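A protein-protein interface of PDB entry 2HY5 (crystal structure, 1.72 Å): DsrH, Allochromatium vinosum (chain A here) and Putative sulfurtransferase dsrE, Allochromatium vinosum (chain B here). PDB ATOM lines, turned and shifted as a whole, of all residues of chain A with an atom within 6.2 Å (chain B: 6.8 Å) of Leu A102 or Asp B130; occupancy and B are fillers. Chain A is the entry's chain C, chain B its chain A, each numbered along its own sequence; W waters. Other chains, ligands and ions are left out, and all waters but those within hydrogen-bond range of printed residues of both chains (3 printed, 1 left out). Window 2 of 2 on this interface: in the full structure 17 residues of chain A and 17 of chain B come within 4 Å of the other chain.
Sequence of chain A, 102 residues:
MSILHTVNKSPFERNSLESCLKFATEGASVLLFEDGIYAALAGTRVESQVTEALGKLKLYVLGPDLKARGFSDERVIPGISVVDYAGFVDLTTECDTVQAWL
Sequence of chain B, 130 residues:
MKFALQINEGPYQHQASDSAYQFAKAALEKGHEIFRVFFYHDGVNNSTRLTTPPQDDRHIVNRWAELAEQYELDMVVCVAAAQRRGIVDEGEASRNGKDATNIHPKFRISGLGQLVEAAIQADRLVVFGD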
ATOM      1  N   THR A   6     -14.978 -23.559 -16.345  1.00  0.00           N
ATOM      2  CA  THR A   6     -13.547 -23.763 -16.521  1.00  0.00           C
ATOM      3  C   THR A   6     -12.829 -22.479 -16.124  1.00  0.00           C
ATOM      4  O   THR A   6     -13.262 -21.379 -16.474  1.00  0.00           O
ATOM      5  CB  THR A   6     -13.180 -24.127 -17.981  1.00  0.00           C
ATOM      6  OG1 THR A   6     -13.564 -23.064 -18.862  1.00  0.00           O
ATOM      7  CG2 THR A   6     -13.881 -25.418 -18.404  1.00  0.00           C
ATOM      8  N   VAL A   7     -11.750 -22.627 -15.367  1.00  0.00           N
ATOM      9  CA  VAL A   7     -10.962 -21.478 -14.913  1.00  0.00           C
ATOM     10  C   VAL A   7      -9.512 -21.753 -15.278  1.00  0.00           C
ATOM     11  O   VAL A   7      -8.927 -22.725 -14.796  1.00  0.00           O
ATOM     12  CB  VAL A   7     -11.075 -21.290 -13.385  1.00  0.00           C
ATOM     13  CG1 VAL A   7     -10.204 -20.124 -12.937  1.00  0.00           C
ATOM     14  CG2 VAL A   7     -12.530 -21.042 -12.999  1.00  0.00           C
ATOM     15  N   ASN A   8      -8.928 -20.902 -16.119  1.00  0.00           N
ATOM     16  CA  ASN A   8      -7.549 -21.122 -16.547  1.00  0.00           C
ATOM     17  C   ASN A   8      -6.540 -20.085 -16.089  1.00  0.00           C
ATOM     18  O   ASN A   8      -5.385 -20.137 -16.494  1.00  0.00           O
ATOM     19  CB  ASN A   8      -7.483 -21.215 -18.073  1.00  0.00           C
ATOM     20  CG  ASN A   8      -7.768 -19.885 -18.749  1.00  0.00           C
ATOM     21  OD1 ASN A   8      -7.332 -19.641 -19.873  1.00  0.00           O
ATOM     22  ND2 ASN A   8      -8.513 -19.021 -18.068  1.00  0.00           N
ATOM     23  N   LYS A   9      -6.973 -19.148 -15.255  1.00  0.00           N
ATOM     24  CA  LYS A   9      -6.085 -18.094 -14.778  1.00  0.00           C
ATOM     25  C   LYS A   9      -5.786 -18.201 -13.292  1.00  0.00           C
ATOM     26  O   LYS A   9      -6.623 -18.641 -12.507  1.00  0.00           O
ATOM     27  CB  LYS A   9      -6.702 -16.727 -15.084  1.00  0.00           C
ATOM     28  CG  LYS A   9      -6.125 -16.041 -16.311  1.00  0.00           C
ATOM     29  CD  LYS A   9      -6.024 -16.980 -17.495  1.00  0.00           C
ATOM     30  CE  LYS A   9      -5.366 -16.310 -18.691  1.00  0.00           C
ATOM     31  NZ  LYS A   9      -3.961 -15.890 -18.447  1.00  0.00           N
ATOM     32  N   ARG A  14      -5.554 -13.103 -11.570  1.00  0.00           N
ATOM     33  CA  ARG A  14      -6.850 -12.636 -12.068  1.00  0.00           C
ATOM     34  C   ARG A  14      -8.005 -12.892 -11.105  1.00  0.00           C
ATOM     35  O   ARG A  14      -7.895 -13.693 -10.172  1.00  0.00           O
ATOM     36  CB  ARG A  14      -7.188 -13.316 -13.397  1.00  0.00           C
ATOM     37  CG  ARG A  14      -7.105 -12.425 -14.621  1.00  0.00           C
ATOM     38  CD  ARG A  14      -5.736 -12.497 -15.264  1.00  0.00           C
ATOM     39  NE  ARG A  14      -5.817 -12.294 -16.707  1.00  0.00           N
ATOM     40  CZ  ARG A  14      -4.779 -12.379 -17.531  1.00  0.00           C
ATOM     41  NH1 ARG A  14      -3.575 -12.663 -17.054  1.00  0.00           N
ATOM     42  NH2 ARG A  14      -4.946 -12.193 -18.833  1.00  0.00           N
ATOM     43  N   SER A  16     -10.831 -14.166 -12.080  1.00  0.00           N
ATOM     44  CA  SER A  16     -11.640 -15.217 -12.691  1.00  0.00           C
ATOM     45  C   SER A  16     -12.170 -16.279 -11.735  1.00  0.00           C
ATOM     46  O   SER A  16     -13.360 -16.598 -11.756  1.00  0.00           O
ATOM     47  CB  SER A  16     -10.846 -15.894 -13.807  1.00  0.00           C
ATOM     48  OG  SER A  16     -10.499 -14.953 -14.803  1.00  0.00           O
ATOM     49  N   GLU A  34      -4.434 -25.058 -16.760  1.00  0.00           N
ATOM     50  CA  GLU A  34      -3.458 -24.025 -17.079  1.00  0.00           C
ATOM     51  C   GLU A  34      -3.047 -23.376 -15.755  1.00  0.00           C
ATOM     52  O   GLU A  34      -2.818 -24.076 -14.770  1.00  0.00           O
ATOM     53  CB  GLU A  34      -4.047 -22.994 -18.052  1.00  0.00           C
ATOM     54  CG  GLU A  34      -4.229 -23.548 -19.460  1.00  0.00           C
ATOM     55  CD  GLU A  34      -4.711 -22.514 -20.460  1.00  0.00           C
ATOM     56  OE1 GLU A  34      -4.517 -21.305 -20.214  1.00  0.00           O
ATOM     57  OE2 GLU A  34      -5.273 -22.915 -21.502  1.00  0.00           O
ATOM     58  N   ALA A 100     -16.683 -20.960 -19.880  1.00  0.00           N
ATOM     59  CA  ALA A 100     -15.291 -20.591 -19.662  1.00  0.00           C
ATOM     60  C   ALA A 100     -15.135 -19.231 -18.986  1.00  0.00           C
ATOM     61  O   ALA A 100     -15.733 -18.244 -19.409  1.00  0.00           O
ATOM     62  CB  ALA A 100     -14.544 -20.594 -20.994  1.00  0.00           C
ATOM     63  N   TRP A 101     -14.338 -19.200 -17.925  1.00  0.00           N
ATOM     64  CA  TRP A 101     -14.050 -17.971 -17.204  1.00  0.00           C
ATOM     65  C   TRP A 101     -12.624 -17.635 -17.584  1.00  0.00           C
ATOM     66  O   TRP A 101     -11.674 -18.212 -17.049  1.00  0.00           O
ATOM     67  CB  TRP A 101     -14.167 -18.173 -15.693  1.00  0.00           C
ATOM     68  CG  TRP A 101     -15.569 -18.425 -15.246  1.00  0.00           C
ATOM     69  CD1 TRP A 101     -16.223 -19.627 -15.220  1.00  0.00           C
ATOM     70  CD2 TRP A 101     -16.509 -17.446 -14.783  1.00  0.00           C
ATOM     71  NE1 TRP A 101     -17.514 -19.457 -14.770  1.00  0.00           N
ATOM     72  CE2 TRP A 101     -17.713 -18.134 -14.492  1.00  0.00           C
ATOM     73  CE3 TRP A 101     -16.449 -16.061 -14.592  1.00  0.00           C
ATOM     74  CZ2 TRP A 101     -18.856 -17.457 -14.003  1.00  0.00           C
ATOM     75  CZ3 TRP A 101     -17.581 -15.397 -14.113  1.00  0.00           C
ATOM     76  CH2 TRP A 101     -18.765 -16.094 -13.824  1.00  0.00           C
ATOM     77  N   LEU A 102     -12.485 -16.716 -18.533  1.00  0.00           N
ATOM     78  CA  LEU A 102     -11.173 -16.317 -19.034  1.00  0.00           C
ATOM     79  C   LEU A 102     -10.505 -15.247 -18.171  1.00  0.00           C
ATOM     80  O   LEU A 102     -10.530 -14.071 -18.586  1.00  0.00           O
ATOM     81  CB  LEU A 102     -11.309 -15.835 -20.486  1.00  0.00           C
ATOM     82  CG  LEU A 102     -11.964 -16.886 -21.401  1.00  0.00           C
ATOM     83  CD1 LEU A 102     -12.078 -16.348 -22.817  1.00  0.00           C
ATOM     84  CD2 LEU A 102     -11.151 -18.176 -21.400  1.00  0.00           C
ATOM     85  OXT LEU A 102      -9.966 -15.591 -17.097  1.00  0.00           O
ATOM     86  N   ASN B   8      -9.205 -18.510 -28.946  1.00  0.00           N
ATOM     87  CA  ASN B   8      -9.080 -17.053 -29.032  1.00  0.00           C
ATOM     88  C   ASN B   8      -7.695 -16.437 -28.955  1.00  0.00           C
ATOM     89  O   ASN B   8      -7.565 -15.215 -29.061  1.00  0.00           O
ATOM     90  CB  ASN B   8      -9.912 -16.388 -27.932  1.00  0.00           C
ATOM     91  CG  ASN B   8     -11.358 -16.835 -27.931  1.00  0.00           C
ATOM     92  OD1 ASN B   8     -11.921 -17.170 -28.971  1.00  0.00           O
ATOM     93  ND2 ASN B   8     -11.977 -16.811 -26.760  1.00  0.00           N
ATOM     94  N   GLU B   9      -6.667 -17.250 -28.765  1.00  0.00           N
ATOM     95  CA  GLU B   9      -5.326 -16.700 -28.642  1.00  0.00           C
ATOM     96  C   GLU B   9      -4.334 -17.266 -29.631  1.00  0.00           C
ATOM     97  O   GLU B   9      -4.492 -18.383 -30.122  1.00  0.00           O
ATOM     98  CB  GLU B   9      -4.805 -16.934 -27.226  1.00  0.00           C
ATOM     99  CG  GLU B   9      -5.747 -16.458 -26.143  1.00  0.00           C
ATOM    100  CD  GLU B   9      -6.113 -14.991 -26.282  1.00  0.00           C
ATOM    101  OE1 GLU B   9      -5.256 -14.204 -26.734  1.00  0.00           O
ATOM    102  OE2 GLU B   9      -7.253 -14.626 -25.920  1.00  0.00           O
ATOM    103  N   GLY B  10      -3.295 -16.482 -29.897  1.00  0.00           N
ATOM    104  CA  GLY B  10      -2.262 -16.901 -30.821  1.00  0.00           C
ATOM    105  C   GLY B  10      -1.396 -18.014 -30.263  1.00  0.00           C
ATOM    106  O   GLY B  10      -1.365 -18.242 -29.049  1.00  0.00           O
ATOM    107  N   GLN B  13       2.193 -17.671 -27.388  1.00  0.00           N
ATOM    108  CA  GLN B  13       1.984 -16.559 -26.457  1.00  0.00           C
ATOM    109  C   GLN B  13       1.128 -16.992 -25.269  1.00  0.00           C
ATOM    110  O   GLN B  13       1.404 -16.628 -24.133  1.00  0.00           O
ATOM    111  CB  GLN B  13       1.309 -15.384 -27.169  1.00  0.00           C
ATOM    112  CG  GLN B  13       1.162 -14.128 -26.302  1.00  0.00           C
ATOM    113  CD  GLN B  13       2.351 -13.187 -26.399  1.00  0.00           C
ATOM    114  OE1 GLN B  13       3.390 -13.526 -26.968  1.00  0.00           O
ATOM    115  NE2 GLN B  13       2.200 -11.991 -25.842  1.00  0.00           N
ATOM    116  N   HIS B  14       0.076 -17.753 -25.550  1.00  0.00           N
ATOM    117  CA  HIS B  14      -0.822 -18.257 -24.513  1.00  0.00           C
ATOM    118  C   HIS B  14      -0.991 -19.760 -24.692  1.00  0.00           C
ATOM    119  O   HIS B  14      -0.921 -20.272 -25.812  1.00  0.00           O
ATOM    120  CB  HIS B  14      -2.188 -17.574 -24.604  1.00  0.00           C
ATOM    121  CG  HIS B  14      -2.159 -16.113 -24.280  1.00  0.00           C
ATOM    122  ND1 HIS B  14      -1.962 -15.139 -25.235  1.00  0.00           N
ATOM    123  CD2 HIS B  14      -2.299 -15.458 -23.101  1.00  0.00           C
ATOM    124  CE1 HIS B  14      -1.984 -13.948 -24.662  1.00  0.00           C
ATOM    125  NE2 HIS B  14      -2.189 -14.114 -23.368  1.00  0.00           N
ATOM    126  N   GLN B  15      -1.219 -20.470 -23.592  1.00  0.00           N
ATOM    127  CA  GLN B  15      -1.373 -21.921 -23.647  1.00  0.00           C
ATOM    128  C   GLN B  15      -2.685 -22.379 -24.284  1.00  0.00           C
ATOM    129  O   GLN B  15      -2.842 -23.555 -24.610  1.00  0.00           O
ATOM    130  CB  GLN B  15      -1.262 -22.500 -22.238  1.00  0.00           C
ATOM    131  CG  GLN B  15      -1.140 -24.019 -22.206  1.00  0.00           C
ATOM    132  CD  GLN B  15      -1.090 -24.565 -20.796  1.00  0.00           C
ATOM    133  OE1 GLN B  15      -0.886 -23.823 -19.831  1.00  0.00           O
ATOM    134  NE2 GLN B  15      -1.264 -25.877 -20.669  1.00  0.00           N
ATOM    135  N   ALA B  16      -3.614 -21.447 -24.469  1.00  0.00           N
ATOM    136  CA  ALA B  16      -4.925 -21.743 -25.049  1.00  0.00           C
ATOM    137  C   ALA B  16      -4.901 -22.719 -26.227  1.00  0.00           C
ATOM    138  O   ALA B  16      -5.588 -23.736 -26.199  1.00  0.00           O
ATOM    139  CB  ALA B  16      -5.616 -20.445 -25.469  1.00  0.00           C
ATOM    140  N   VAL B 127     -14.669 -23.187 -25.184  1.00  0.00           N
ATOM    141  CA  VAL B 127     -13.851 -22.034 -25.539  1.00  0.00           C
ATOM    142  C   VAL B 127     -12.525 -22.000 -24.791  1.00  0.00           C
ATOM    143  O   VAL B 127     -12.472 -22.197 -23.578  1.00  0.00           O
ATOM    144  CB  VAL B 127     -14.611 -20.720 -25.249  1.00  0.00           C
ATOM    145  CG1 VAL B 127     -13.797 -19.523 -25.750  1.00  0.00           C
ATOM    146  CG2 VAL B 127     -15.977 -20.751 -25.914  1.00  0.00           C
ATOM    147  N   PHE B 128     -11.454 -21.747 -25.532  1.00  0.00           N
ATOM    148  CA  PHE B 128     -10.122 -21.678 -24.955  1.00  0.00           C
ATOM    149  C   PHE B 128      -9.564 -20.294 -25.218  1.00  0.00           C
ATOM    150  O   PHE B 128      -9.436 -19.877 -26.366  1.00  0.00           O
ATOM    151  CB  PHE B 128      -9.211 -22.737 -25.585  1.00  0.00           C
ATOM    152  CG  PHE B 128      -9.616 -24.150 -25.267  1.00  0.00           C
ATOM    153  CD1 PHE B 128     -10.619 -24.785 -25.999  1.00  0.00           C
ATOM    154  CD2 PHE B 128      -9.024 -24.832 -24.209  1.00  0.00           C
ATOM    155  CE1 PHE B 128     -11.027 -26.083 -25.680  1.00  0.00           C
ATOM    156  CE2 PHE B 128      -9.426 -26.136 -23.878  1.00  0.00           C
ATOM    157  CZ  PHE B 128     -10.430 -26.759 -24.616  1.00  0.00           C
ATOM    158  N   GLY B 129      -9.239 -19.576 -24.152  1.00  0.00           N
ATOM    159  CA  GLY B 129      -8.712 -18.238 -24.325  1.00  0.00           C
ATOM    160  C   GLY B 129      -7.856 -17.801 -23.161  1.00  0.00           C
ATOM    161  O   GLY B 129      -7.220 -18.624 -22.505  1.00  0.00           O
ATOM    162  N   ASP B 130      -7.858 -16.494 -22.910  1.00  0.00           N
ATOM    163  CA  ASP B 130      -7.087 -15.890 -21.825  1.00  0.00           C
ATOM    164  C   ASP B 130      -7.993 -15.428 -20.700  1.00  0.00           C
ATOM    165  O   ASP B 130      -8.577 -14.328 -20.827  1.00  0.00           O
ATOM    166  CB  ASP B 130      -6.291 -14.698 -22.345  1.00  0.00           C
ATOM    167  CG  ASP B 130      -5.265 -15.101 -23.363  1.00  0.00           C
ATOM    168  OD1 ASP B 130      -4.705 -14.204 -24.030  1.00  0.00           O
ATOM    169  OD2 ASP B 130      -5.010 -16.319 -23.487  1.00  0.00           O
ATOM    170  OXT ASP B 130      -8.113 -16.167 -19.705  1.00  0.00           O
HETATM  171  O   HOH W   1      -7.777 -21.824 -22.365  1.00  0.00           O
HETATM  172  O   HOH W   2      -2.937 -17.507 -21.161  1.00  0.00           O
HETATM  173  O   HOH W   3     -14.066 -23.818 -21.646  1.00  0.00           O
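O of Gly B129 lies close to OD1 of Asn A8, 2.8 Å away. OXT of Asp B130 lies within hydrogen-bond range of ND2 of Asn A8, 3.3 Å away. The chain-end carboxylate (O) of Leu A102 sits close to the chain-end carboxylate (O) of Asp B130 (3.0 Å).
N of Asn B8 lies within hydrogen-bond range of O of Phe B128 (2.9 Å). A ring nitrogen (NE2) of His B14 lies within hydrogen-bond range of the side-chain carboxylate (OD1) of Asp B130 (2.6 Å). The side-chain amide oxygen (OD1) of Asn A8 lies close to the side-chain carboxylate (OE1) of Glu A34, at 3.3 Å. The backbone carbonyl oxygen of Trp A101 sits at hydrogen-bond distance from the side-chain amide nitrogen of Asn A8 (3.4 Å). The side-chain hydroxyl (OG) of Ser A16 sits at hydrogen-bond distance from the chain-end carboxylate (OXT) of Leu A102, 2.4 Å away.
Lys A9 touches Asp B130 (CE to OXT, 2.9 Å). CG of Glu A34 touches OE1 of Gln B15, at 3.4 Å. Glu A34 touches Ala B16 (OE2 to N, 3.7 Å). Val B127 touches Ala A100. Leu A102 touches Asn B8. Gly B129 touches Leu A102.
Printed residues of chain B within 4 Å of Leu A102: Asn B8, Gly B129 and Asp B130. Asp B130 touches just these residues of chain A: Asn A8 (3.3 Å), Lys A9 (2.9 Å) and Leu A102 (3.0 Å). Printed residues of chain A within 4 Å of Gly B129: Asn A8 and Leu A102. Printed residues of chain A within 4 Å of Asn B8: Leu A102 (3.97 Å). The nearest residue of chain A that does not touch Asp B130 is Arg A14 (4.5 Å).
Of the 11 printed residues of chain B, 6 touch a printed residue of chain A. Of the 10 printed residues of chain A, 5 touch a printed residue of chain B. Among the printed residues, no Asp or Glu carboxylate lies within 4 Å of a Lys or Arg side-chain nitrogen of the other chain.
Water W1 lies within hydrogen-bond range of the side-chain carboxylate of Glu A34 (2.9 Å), the backbone NH of Gly B129 (3.2 Å) and the side-chain amide oxygen of Asn A8 (3.3 Å). Water W3 bridges the side-chain hydroxyl (OG1) of Thr A6 (2.9 Å) and the backbone carbonyl oxygen (O) of Val B127 (3.0 Å). Water W2 bridges NZ of Lys A9 (3.3 Å) and OD2 of Asp B130 (3.3 Å).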
